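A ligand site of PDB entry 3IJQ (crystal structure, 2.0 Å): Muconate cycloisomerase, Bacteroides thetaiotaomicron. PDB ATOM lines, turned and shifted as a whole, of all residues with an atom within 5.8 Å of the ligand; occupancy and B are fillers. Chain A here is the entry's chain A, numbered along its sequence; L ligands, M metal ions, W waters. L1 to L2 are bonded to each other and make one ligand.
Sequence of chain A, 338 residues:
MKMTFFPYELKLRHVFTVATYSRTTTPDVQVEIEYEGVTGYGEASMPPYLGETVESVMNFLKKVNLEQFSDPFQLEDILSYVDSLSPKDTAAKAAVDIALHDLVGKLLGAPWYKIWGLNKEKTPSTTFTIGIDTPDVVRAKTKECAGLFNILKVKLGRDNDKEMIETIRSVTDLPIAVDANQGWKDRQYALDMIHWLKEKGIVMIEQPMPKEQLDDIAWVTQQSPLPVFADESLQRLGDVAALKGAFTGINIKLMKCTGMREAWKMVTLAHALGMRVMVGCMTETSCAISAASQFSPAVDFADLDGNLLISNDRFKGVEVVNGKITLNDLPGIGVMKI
Water W2 lies within hydrogen-bond range of OG1 of Thr 129 (2.6 Å), OD2 of Asp 305 (2.8 Å), N1 of LIG L1 (2.8 Å) and OD1 of Asp 303 (3.1 Å).
Water W1 bridges the side-chain amino group of Lys 153 (3.0 Å) and an oxygen (O1) of LG2 L2 (3.4 Å).
CE2 of Phe 16 touches C4 of LG2 L2 (3.4 Å).
CB of Pro 47 touches O2 of LG2 L2 (3.2 Å).
Lys 153 touches the ligand.
CA of Met 282 touches O3 of LG2 L2 (3.3 Å).
CD1 of Leu 309 touches C3 of LIG L1, at 3.6 Å.
Hydrophobic or aromatic side chains within 4 Å of the ligand: Phe 16, Pro 47, Tyr 49, Met 282 and Leu 309.
12 residues have an atom within 4 Å of the ligand: Phe 16, Arg 23, Pro 47, Tyr 49, Lys 153, Lys 253, Cys 281, Met 282, Thr 283, Asp 303, Asp 305 and Leu 309.
The nearest printed residue that does not touch the ligand is Val 18 (4.01 Å).
OD1 of Asp 305 is in salt-bridge range of N1 of LIG L1 (2.6 Å).
NH2 of Arg 23 is in salt-bridge range of O2 of LG2 L2, at 2.7 Å.
A nitrogen (N1) of LIG L1 is in salt-bridge range of the side-chain carboxylate (OD2) of Asp 303 (2.8 Å).
The backbone carbonyl oxygen (O) of Cys 281 is in hydrogen-bond range of a nitrogen (N1) of LG2 L2.
N of Thr 283 is in hydrogen-bond range of O3 of LG2 L2, at 3.0 Å.
The side-chain hydroxyl of Tyr 49 is in hydrogen-bond range of an oxygen (O2) of LG2 L2, 3.0 Å away.
The side-chain amino group (NZ) of Lys 253 lies within salt-bridge range of an oxygen (O4) of LG2 L2 (3.3 Å).
The backbone carbonyl oxygen (O) of Arg 23 is in hydrogen-bond range of the backbone NH (N) of Phe 16, 2.7 Å away.
OG1 of Thr 26 sits at hydrogen-bond distance from NE of Arg 23 (3.0 Å).
The backbone carbonyl oxygen of Asp 303 lies within hydrogen-bond range of the side-chain sulfur of Cys 281 (3.3 Å).
The side-chain carboxylate (OD2) of Asp 303 lies within salt-bridge range of the side-chain amino group (NZ) of Lys 153 (3.0 Å).
The backbone NH (N) of Gly 306 is in hydrogen-bond range of the side-chain sulfur (SG) of Cys 281 (3.4 Å).
The backbone carbonyl oxygen (O) of Thr 283 lies within hydrogen-bond range of the side-chain hydroxyl (OG) of Ser 45 (2.8 Å).
The side-chain hydroxyl (OG1) of Thr 26 sits at hydrogen-bond distance from the side-chain hydroxyl (OG1) of Thr 283.
The side-chain amino group (NZ) of Lys 253 lies within salt-bridge range of the side-chain carboxylate (OD1) of Asp 231 (2.7 Å).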
ATOM      1  N   PHE A  16     -32.037 -13.974 -33.714  1.00  0.00           N
ATOM      2  CA  PHE A  16     -30.775 -13.292 -33.497  1.00  0.00           C
ATOM      3  C   PHE A  16     -29.712 -14.368 -33.313  1.00  0.00           C
ATOM      4  O   PHE A  16     -29.872 -15.274 -32.489  1.00  0.00           O
ATOM      5  CB  PHE A  16     -30.838 -12.399 -32.257  1.00  0.00           C
ATOM      6  CG  PHE A  16     -29.727 -11.388 -32.195  1.00  0.00           C
ATOM      7  CD1 PHE A  16     -29.660 -10.358 -33.133  1.00  0.00           C
ATOM      8  CD2 PHE A  16     -28.745 -11.470 -31.221  1.00  0.00           C
ATOM      9  CE1 PHE A  16     -28.629  -9.429 -33.110  1.00  0.00           C
ATOM     10  CE2 PHE A  16     -27.711 -10.541 -31.188  1.00  0.00           C
ATOM     11  CZ  PHE A  16     -27.648  -9.523 -32.123  1.00  0.00           C
ATOM     12  N   VAL A  18     -25.475 -15.207 -32.829  1.00  0.00           N
ATOM     13  CA  VAL A  18     -24.125 -14.762 -32.502  1.00  0.00           C
ATOM     14  C   VAL A  18     -23.259 -16.011 -32.350  1.00  0.00           C
ATOM     15  O   VAL A  18     -23.617 -16.946 -31.621  1.00  0.00           O
ATOM     16  CB  VAL A  18     -24.099 -13.949 -31.194  1.00  0.00           C
ATOM     17  CG1 VAL A  18     -24.821 -12.629 -31.400  1.00  0.00           C
ATOM     18  CG2 VAL A  18     -24.751 -14.735 -30.077  1.00  0.00           C
ATOM     19  N   ARG A  23     -31.187 -17.258 -31.146  1.00  0.00           N
ATOM     20  CA  ARG A  23     -32.323 -17.185 -30.247  1.00  0.00           C
ATOM     21  C   ARG A  23     -33.323 -16.184 -30.800  1.00  0.00           C
ATOM     22  O   ARG A  23     -33.036 -15.457 -31.744  1.00  0.00           O
ATOM     23  CB  ARG A  23     -31.857 -16.760 -28.844  1.00  0.00           C
ATOM     24  CG  ARG A  23     -31.186 -15.385 -28.779  1.00  0.00           C
ATOM     25  CD  ARG A  23     -30.910 -15.009 -27.321  1.00  0.00           C
ATOM     26  NE  ARG A  23     -30.660 -13.587 -27.123  1.00  0.00           N
ATOM     27  CZ  ARG A  23     -29.533 -12.962 -27.437  1.00  0.00           C
ATOM     28  NH1 ARG A  23     -28.519 -13.624 -27.967  1.00  0.00           N
ATOM     29  NH2 ARG A  23     -29.430 -11.656 -27.220  1.00  0.00           N
ATOM     30  N   THR A  26     -34.725 -12.909 -25.159  1.00  0.00           N
ATOM     31  CA  THR A  26     -33.587 -12.534 -24.325  1.00  0.00           C
ATOM     32  C   THR A  26     -34.020 -12.315 -22.892  1.00  0.00           C
ATOM     33  O   THR A  26     -34.869 -11.467 -22.617  1.00  0.00           O
ATOM     34  CB  THR A  26     -32.908 -11.234 -24.812  1.00  0.00           C
ATOM     35  OG1 THR A  26     -32.452 -11.386 -26.156  1.00  0.00           O
ATOM     36  CG2 THR A  26     -31.702 -10.904 -23.920  1.00  0.00           C
ATOM     37  N   SER A  45     -30.160  -6.850 -19.131  1.00  0.00           N
ATOM     38  CA  SER A  45     -30.377  -7.726 -20.277  1.00  0.00           C
ATOM     39  C   SER A  45     -29.356  -8.832 -20.150  1.00  0.00           C
ATOM     40  O   SER A  45     -28.187  -8.565 -19.849  1.00  0.00           O
ATOM     41  CB  SER A  45     -30.153  -6.980 -21.584  1.00  0.00           C
ATOM     42  OG  SER A  45     -30.154  -7.873 -22.679  1.00  0.00           O
ATOM     43  N   PRO A  47     -28.001 -11.846 -22.424  1.00  0.00           N
ATOM     44  CA  PRO A  47     -27.904 -12.803 -23.530  1.00  0.00           C
ATOM     45  C   PRO A  47     -27.520 -14.109 -22.853  1.00  0.00           C
ATOM     46  O   PRO A  47     -26.462 -14.203 -22.227  1.00  0.00           O
ATOM     47  CB  PRO A  47     -26.765 -12.218 -24.369  1.00  0.00           C
ATOM     48  CG  PRO A  47     -26.956 -10.745 -24.179  1.00  0.00           C
ATOM     49  CD  PRO A  47     -27.226 -10.626 -22.698  1.00  0.00           C
ATOM     50  N   TYR A  49     -25.848 -16.414 -23.115  1.00  0.00           N
ATOM     51  CA  TYR A  49     -24.529 -16.977 -23.362  1.00  0.00           C
ATOM     52  C   TYR A  49     -23.478 -16.118 -22.682  1.00  0.00           C
ATOM     53  O   TYR A  49     -22.289 -16.209 -22.994  1.00  0.00           O
ATOM     54  CB  TYR A  49     -24.268 -17.055 -24.877  1.00  0.00           C
ATOM     55  CG  TYR A  49     -24.161 -15.709 -25.573  1.00  0.00           C
ATOM     56  CD1 TYR A  49     -23.000 -14.952 -25.493  1.00  0.00           C
ATOM     57  CD2 TYR A  49     -25.231 -15.196 -26.303  1.00  0.00           C
ATOM     58  CE1 TYR A  49     -22.894 -13.719 -26.122  1.00  0.00           C
ATOM     59  CE2 TYR A  49     -25.141 -13.959 -26.938  1.00  0.00           C
ATOM     60  CZ  TYR A  49     -23.970 -13.231 -26.837  1.00  0.00           C
ATOM     61  OH  TYR A  49     -23.859 -12.007 -27.465  1.00  0.00           O
ATOM     62  N   THR A 129     -26.653  -4.128 -37.975  1.00  0.00           N
ATOM     63  CA  THR A 129     -26.042  -5.333 -38.542  1.00  0.00           C
ATOM     64  C   THR A 129     -26.696  -5.942 -39.778  1.00  0.00           C
ATOM     65  O   THR A 129     -27.919  -6.028 -39.886  1.00  0.00           O
ATOM     66  CB  THR A 129     -25.926  -6.443 -37.470  1.00  0.00           C
ATOM     67  OG1 THR A 129     -24.921  -6.090 -36.519  1.00  0.00           O
ATOM     68  CG2 THR A 129     -25.564  -7.779 -38.122  1.00  0.00           C
ATOM     69  N   LYS A 153     -22.846  -2.509 -39.658  1.00  0.00           N
ATOM     70  CA  LYS A 153     -22.009  -3.438 -38.907  1.00  0.00           C
ATOM     71  C   LYS A 153     -22.084  -4.833 -39.511  1.00  0.00           C
ATOM     72  O   LYS A 153     -23.162  -5.299 -39.897  1.00  0.00           O
ATOM     73  CB  LYS A 153     -22.457  -3.484 -37.455  1.00  0.00           C
ATOM     74  CG  LYS A 153     -21.708  -4.491 -36.603  1.00  0.00           C
ATOM     75  CD  LYS A 153     -22.189  -4.453 -35.162  1.00  0.00           C
ATOM     76  CE  LYS A 153     -21.427  -5.431 -34.297  1.00  0.00           C
ATOM     77  NZ  LYS A 153     -21.947  -5.422 -32.904  1.00  0.00           N
ATOM     78  N   LYS A 155     -20.544  -8.870 -38.806  1.00  0.00           N
ATOM     79  CA  LYS A 155     -19.765  -9.817 -38.014  1.00  0.00           C
ATOM     80  C   LYS A 155     -18.921 -10.723 -38.913  1.00  0.00           C
ATOM     81  O   LYS A 155     -19.442 -11.681 -39.501  1.00  0.00           O
ATOM     82  CB  LYS A 155     -20.691 -10.677 -37.129  1.00  0.00           C
ATOM     83  CG  LYS A 155     -21.392  -9.905 -36.024  1.00  0.00           C
ATOM     84  CD  LYS A 155     -22.750  -9.370 -36.489  1.00  0.00           C
ATOM     85  CE  LYS A 155     -23.841 -10.420 -36.330  1.00  0.00           C
ATOM     86  NZ  LYS A 155     -24.139 -10.704 -34.893  1.00  0.00           N
ATOM     87  N   ASP A 179     -17.089  -6.744 -36.851  1.00  0.00           N
ATOM     88  CA  ASP A 179     -16.836  -7.335 -35.543  1.00  0.00           C
ATOM     89  C   ASP A 179     -16.356  -8.767 -35.754  1.00  0.00           C
ATOM     90  O   ASP A 179     -17.177  -9.666 -35.993  1.00  0.00           O
ATOM     91  CB  ASP A 179     -18.115  -7.331 -34.706  1.00  0.00           C
ATOM     92  CG  ASP A 179     -17.854  -7.609 -33.242  1.00  0.00           C
ATOM     93  OD1 ASP A 179     -16.800  -8.190 -32.930  1.00  0.00           O
ATOM     94  OD2 ASP A 179     -18.707  -7.230 -32.407  1.00  0.00           O
ATOM     95  N   ASN A 181     -14.908 -10.838 -33.531  1.00  0.00           N
ATOM     96  CA  ASN A 181     -15.190 -11.710 -32.390  1.00  0.00           C
ATOM     97  C   ASN A 181     -14.076 -12.717 -32.135  1.00  0.00           C
ATOM     98  O   ASN A 181     -14.342 -13.898 -31.928  1.00  0.00           O
ATOM     99  CB  ASN A 181     -16.498 -12.469 -32.614  1.00  0.00           C
ATOM    100  CG  ASN A 181     -17.690 -11.547 -32.812  1.00  0.00           C
ATOM    101  OD1 ASN A 181     -18.154 -10.900 -31.869  1.00  0.00           O
ATOM    102  ND2 ASN A 181     -18.184 -11.477 -34.040  1.00  0.00           N
ATOM    103  N   GLU A 206     -13.211  -4.612 -34.921  1.00  0.00           N
ATOM    104  CA  GLU A 206     -13.500  -4.902 -33.528  1.00  0.00           C
ATOM    105  C   GLU A 206     -13.094  -6.303 -33.109  1.00  0.00           C
ATOM    106  O   GLU A 206     -13.572  -7.284 -33.675  1.00  0.00           O
ATOM    107  CB  GLU A 206     -15.001  -4.706 -33.250  1.00  0.00           C
ATOM    108  CG  GLU A 206     -15.518  -5.351 -31.961  1.00  0.00           C
ATOM    109  CD  GLU A 206     -16.970  -5.010 -31.675  1.00  0.00           C
ATOM    110  OE1 GLU A 206     -17.571  -5.633 -30.775  1.00  0.00           O
ATOM    111  OE2 GLU A 206     -17.507  -4.103 -32.347  1.00  0.00           O
ATOM    112  N   ASP A 231     -13.343  -5.707 -27.310  1.00  0.00           N
ATOM    113  CA  ASP A 231     -14.670  -5.978 -26.781  1.00  0.00           C
ATOM    114  C   ASP A 231     -14.591  -7.127 -25.767  1.00  0.00           C
ATOM    115  O   ASP A 231     -14.841  -6.937 -24.576  1.00  0.00           O
ATOM    116  CB  ASP A 231     -15.624  -6.357 -27.914  1.00  0.00           C
ATOM    117  CG  ASP A 231     -17.041  -6.626 -27.431  1.00  0.00           C
ATOM    118  OD1 ASP A 231     -17.247  -6.783 -26.208  1.00  0.00           O
ATOM    119  OD2 ASP A 231     -17.951  -6.690 -28.281  1.00  0.00           O
ATOM    120  N   GLU A 232     -14.249  -8.309 -26.264  1.00  0.00           N
ATOM    121  CA  GLU A 232     -14.129  -9.491 -25.406  1.00  0.00           C
ATOM    122  C   GLU A 232     -12.900  -9.373 -24.513  1.00  0.00           C
ATOM    123  O   GLU A 232     -12.832  -9.983 -23.441  1.00  0.00           O
ATOM    124  CB  GLU A 232     -14.007 -10.763 -26.266  1.00  0.00           C
ATOM    125  CG  GLU A 232     -15.306 -11.255 -26.898  1.00  0.00           C
ATOM    126  CD  GLU A 232     -15.838 -10.337 -27.984  1.00  0.00           C
ATOM    127  OE1 GLU A 232     -15.030  -9.826 -28.797  1.00  0.00           O
ATOM    128  OE2 GLU A 232     -17.076 -10.141 -28.041  1.00  0.00           O
ATOM    129  N   ASN A 251     -14.418  -0.917 -26.307  1.00  0.00           N
ATOM    130  CA  ASN A 251     -15.856  -0.894 -26.500  1.00  0.00           C
ATOM    131  C   ASN A 251     -16.493  -1.076 -25.140  1.00  0.00           C
ATOM    132  O   ASN A 251     -16.161  -2.018 -24.400  1.00  0.00           O
ATOM    133  CB  ASN A 251     -16.284  -2.034 -27.429  1.00  0.00           C
ATOM    134  CG  ASN A 251     -17.789  -2.191 -27.504  1.00  0.00           C
ATOM    135  OD1 ASN A 251     -18.514  -1.238 -27.798  1.00  0.00           O
ATOM    136  ND2 ASN A 251     -18.272  -3.402 -27.226  1.00  0.00           N
ATOM    137  N   LYS A 253     -19.934  -1.593 -22.714  1.00  0.00           N
ATOM    138  CA  LYS A 253     -21.306  -2.077 -22.681  1.00  0.00           C
ATOM    139  C   LYS A 253     -21.782  -2.058 -21.219  1.00  0.00           C
ATOM    140  O   LYS A 253     -21.169  -2.687 -20.354  1.00  0.00           O
ATOM    141  CB  LYS A 253     -21.400  -3.482 -23.289  1.00  0.00           C
ATOM    142  CG  LYS A 253     -20.858  -3.536 -24.714  1.00  0.00           C
ATOM    143  CD  LYS A 253     -21.584  -4.566 -25.567  1.00  0.00           C
ATOM    144  CE  LYS A 253     -20.875  -5.911 -25.586  1.00  0.00           C
ATOM    145  NZ  LYS A 253     -19.778  -5.990 -26.599  1.00  0.00           N
ATOM    146  N   GLY A 280     -21.472  -0.085 -26.997  1.00  0.00           N
ATOM    147  CA  GLY A 280     -22.306  -1.095 -27.608  1.00  0.00           C
ATOM    148  C   GLY A 280     -23.460  -1.433 -26.702  1.00  0.00           C
ATOM    149  O   GLY A 280     -23.722  -0.722 -25.734  1.00  0.00           O
ATOM    150  N   CYS A 281     -24.128  -2.535 -26.993  1.00  0.00           N
ATOM    151  CA  CYS A 281     -25.271  -2.931 -26.199  1.00  0.00           C
ATOM    152  C   CYS A 281     -25.659  -4.352 -26.513  1.00  0.00           C
ATOM    153  O   CYS A 281     -25.113  -4.959 -27.434  1.00  0.00           O
ATOM    154  CB  CYS A 281     -26.472  -2.055 -26.546  1.00  0.00           C
ATOM    155  SG  CYS A 281     -27.036  -2.288 -28.271  1.00  0.00           S
ATOM    156  N   MET A 282     -26.598  -4.871 -25.744  1.00  0.00           N
ATOM    157  CA  MET A 282     -27.149  -6.196 -25.957  1.00  0.00           C
ATOM    158  C   MET A 282     -28.536  -5.841 -26.484  1.00  0.00           C
ATOM    159  O   MET A 282     -28.890  -4.665 -26.562  1.00  0.00           O
ATOM    160  CB  MET A 282     -27.322  -6.939 -24.635  1.00  0.00           C
ATOM    161  CG  MET A 282     -26.149  -6.872 -23.676  1.00  0.00           C
ATOM    162  SD  MET A 282     -24.747  -7.857 -24.198  1.00  0.00           S
ATOM    163  CE  MET A 282     -23.913  -6.717 -25.176  1.00  0.00           C
ATOM    164  N   THR A 283     -29.328  -6.835 -26.868  1.00  0.00           N
ATOM    165  CA  THR A 283     -30.682  -6.544 -27.301  1.00  0.00           C
ATOM    166  C   THR A 283     -31.248  -6.054 -25.990  1.00  0.00           C
ATOM    167  O   THR A 283     -31.200  -6.773 -24.991  1.00  0.00           O
ATOM    168  CB  THR A 283     -31.414  -7.819 -27.740  1.00  0.00           C
ATOM    169  OG1 THR A 283     -31.327  -8.798 -26.698  1.00  0.00           O
ATOM    170  CG2 THR A 283     -30.788  -8.380 -29.019  1.00  0.00           C
ATOM    171  N   ASP A 303     -22.756   1.370 -31.362  1.00  0.00           N
ATOM    172  CA  ASP A 303     -23.593   0.289 -31.825  1.00  0.00           C
ATOM    173  C   ASP A 303     -24.719   0.275 -30.791  1.00  0.00           C
ATOM    174  O   ASP A 303     -24.732  -0.550 -29.876  1.00  0.00           O
ATOM    175  CB  ASP A 303     -22.826  -1.039 -31.822  1.00  0.00           C
ATOM    176  CG  ASP A 303     -23.617  -2.173 -32.451  1.00  0.00           C
ATOM    177  OD1 ASP A 303     -24.118  -1.986 -33.577  1.00  0.00           O
ATOM    178  OD2 ASP A 303     -23.745  -3.238 -31.817  1.00  0.00           O
ATOM    179  N   ASP A 305     -28.302  -0.025 -31.262  1.00  0.00           N
ATOM    180  CA  ASP A 305     -29.513  -0.337 -32.018  1.00  0.00           C
ATOM    181  C   ASP A 305     -30.306  -1.462 -31.350  1.00  0.00           C
ATOM    182  O   ASP A 305     -31.279  -1.973 -31.922  1.00  0.00           O
ATOM    183  CB  ASP A 305     -29.118  -0.752 -33.435  1.00  0.00           C
ATOM    184  CG  ASP A 305     -28.280  -2.023 -33.450  1.00  0.00           C
ATOM    185  OD1 ASP A 305     -27.840  -2.451 -32.369  1.00  0.00           O
ATOM    186  OD2 ASP A 305     -28.076  -2.594 -34.545  1.00  0.00           O
ATOM    187  N   GLY A 306     -29.891  -1.838 -30.141  1.00  0.00           N
ATOM    188  CA  GLY A 306     -30.530  -2.911 -29.402  1.00  0.00           C
ATOM    189  C   GLY A 306     -32.048  -2.909 -29.398  1.00  0.00           C
ATOM    190  O   GLY A 306     -32.683  -3.893 -29.789  1.00  0.00           O
ATOM    191  N   LEU A 309     -34.045  -4.068 -32.342  1.00  0.00           N
ATOM    192  CA  LEU A 309     -34.120  -5.503 -32.593  1.00  0.00           C
ATOM    193  C   LEU A 309     -35.230  -6.240 -31.847  1.00  0.00           C
ATOM    194  O   LEU A 309     -35.538  -7.387 -32.149  1.00  0.00           O
ATOM    195  CB  LEU A 309     -32.765  -6.148 -32.281  1.00  0.00           C
ATOM    196  CG  LEU A 309     -31.589  -5.546 -33.061  1.00  0.00           C
ATOM    197  CD1 LEU A 309     -30.274  -6.092 -32.539  1.00  0.00           C
ATOM    198  CD2 LEU A 309     -31.744  -5.851 -34.544  1.00  0.00           C
HETATM  199  N1  LIG L   1     -26.177  -4.398 -32.370  1.00  0.00           N
HETATM  200  C1  LIG L   1     -26.047  -5.049 -31.058  1.00  0.00           C
HETATM  201  C2  LIG L   1     -25.205  -6.342 -30.998  1.00  0.00           C
HETATM  202  O1  LIG L   1     -24.999  -7.024 -31.984  1.00  0.00           O
HETATM  203  C3  LIG L   1     -27.420  -5.343 -30.491  1.00  0.00           C
HETATM  204  N1  LG2 L   2     -24.727  -6.631 -29.788  1.00  0.00           N
HETATM  205  C1  LG2 L   2     -23.960  -7.864 -29.503  1.00  0.00           C
HETATM  206  C2  LG2 L   2     -22.471  -7.574 -29.230  1.00  0.00           C
HETATM  207  O1  LG2 L   2     -21.674  -8.517 -29.392  1.00  0.00           O
HETATM  208  C3  LG2 L   2     -24.609  -8.583 -28.321  1.00  0.00           C
HETATM  209  C4  LG2 L   2     -25.539  -9.699 -28.762  1.00  0.00           C
HETATM  210  C5  LG2 L   2     -26.678 -10.007 -27.811  1.00  0.00           C
HETATM  211  O2  LG2 L   2     -26.790 -11.172 -27.391  1.00  0.00           O
HETATM  212  O3  LG2 L   2     -27.460  -9.093 -27.491  1.00  0.00           O
HETATM  213  O4  LG2 L   2     -22.129  -6.432 -28.875  1.00  0.00           O
HETATM  214 MG    MG M   1     -18.801  -7.039 -30.136  1.00  0.00          MG
HETATM  215  O   HOH W   1     -21.068  -8.292 -32.699  1.00  0.00           O
HETATM  216  O   HOH W   2     -25.774  -4.038 -35.157  1.00  0.00           O
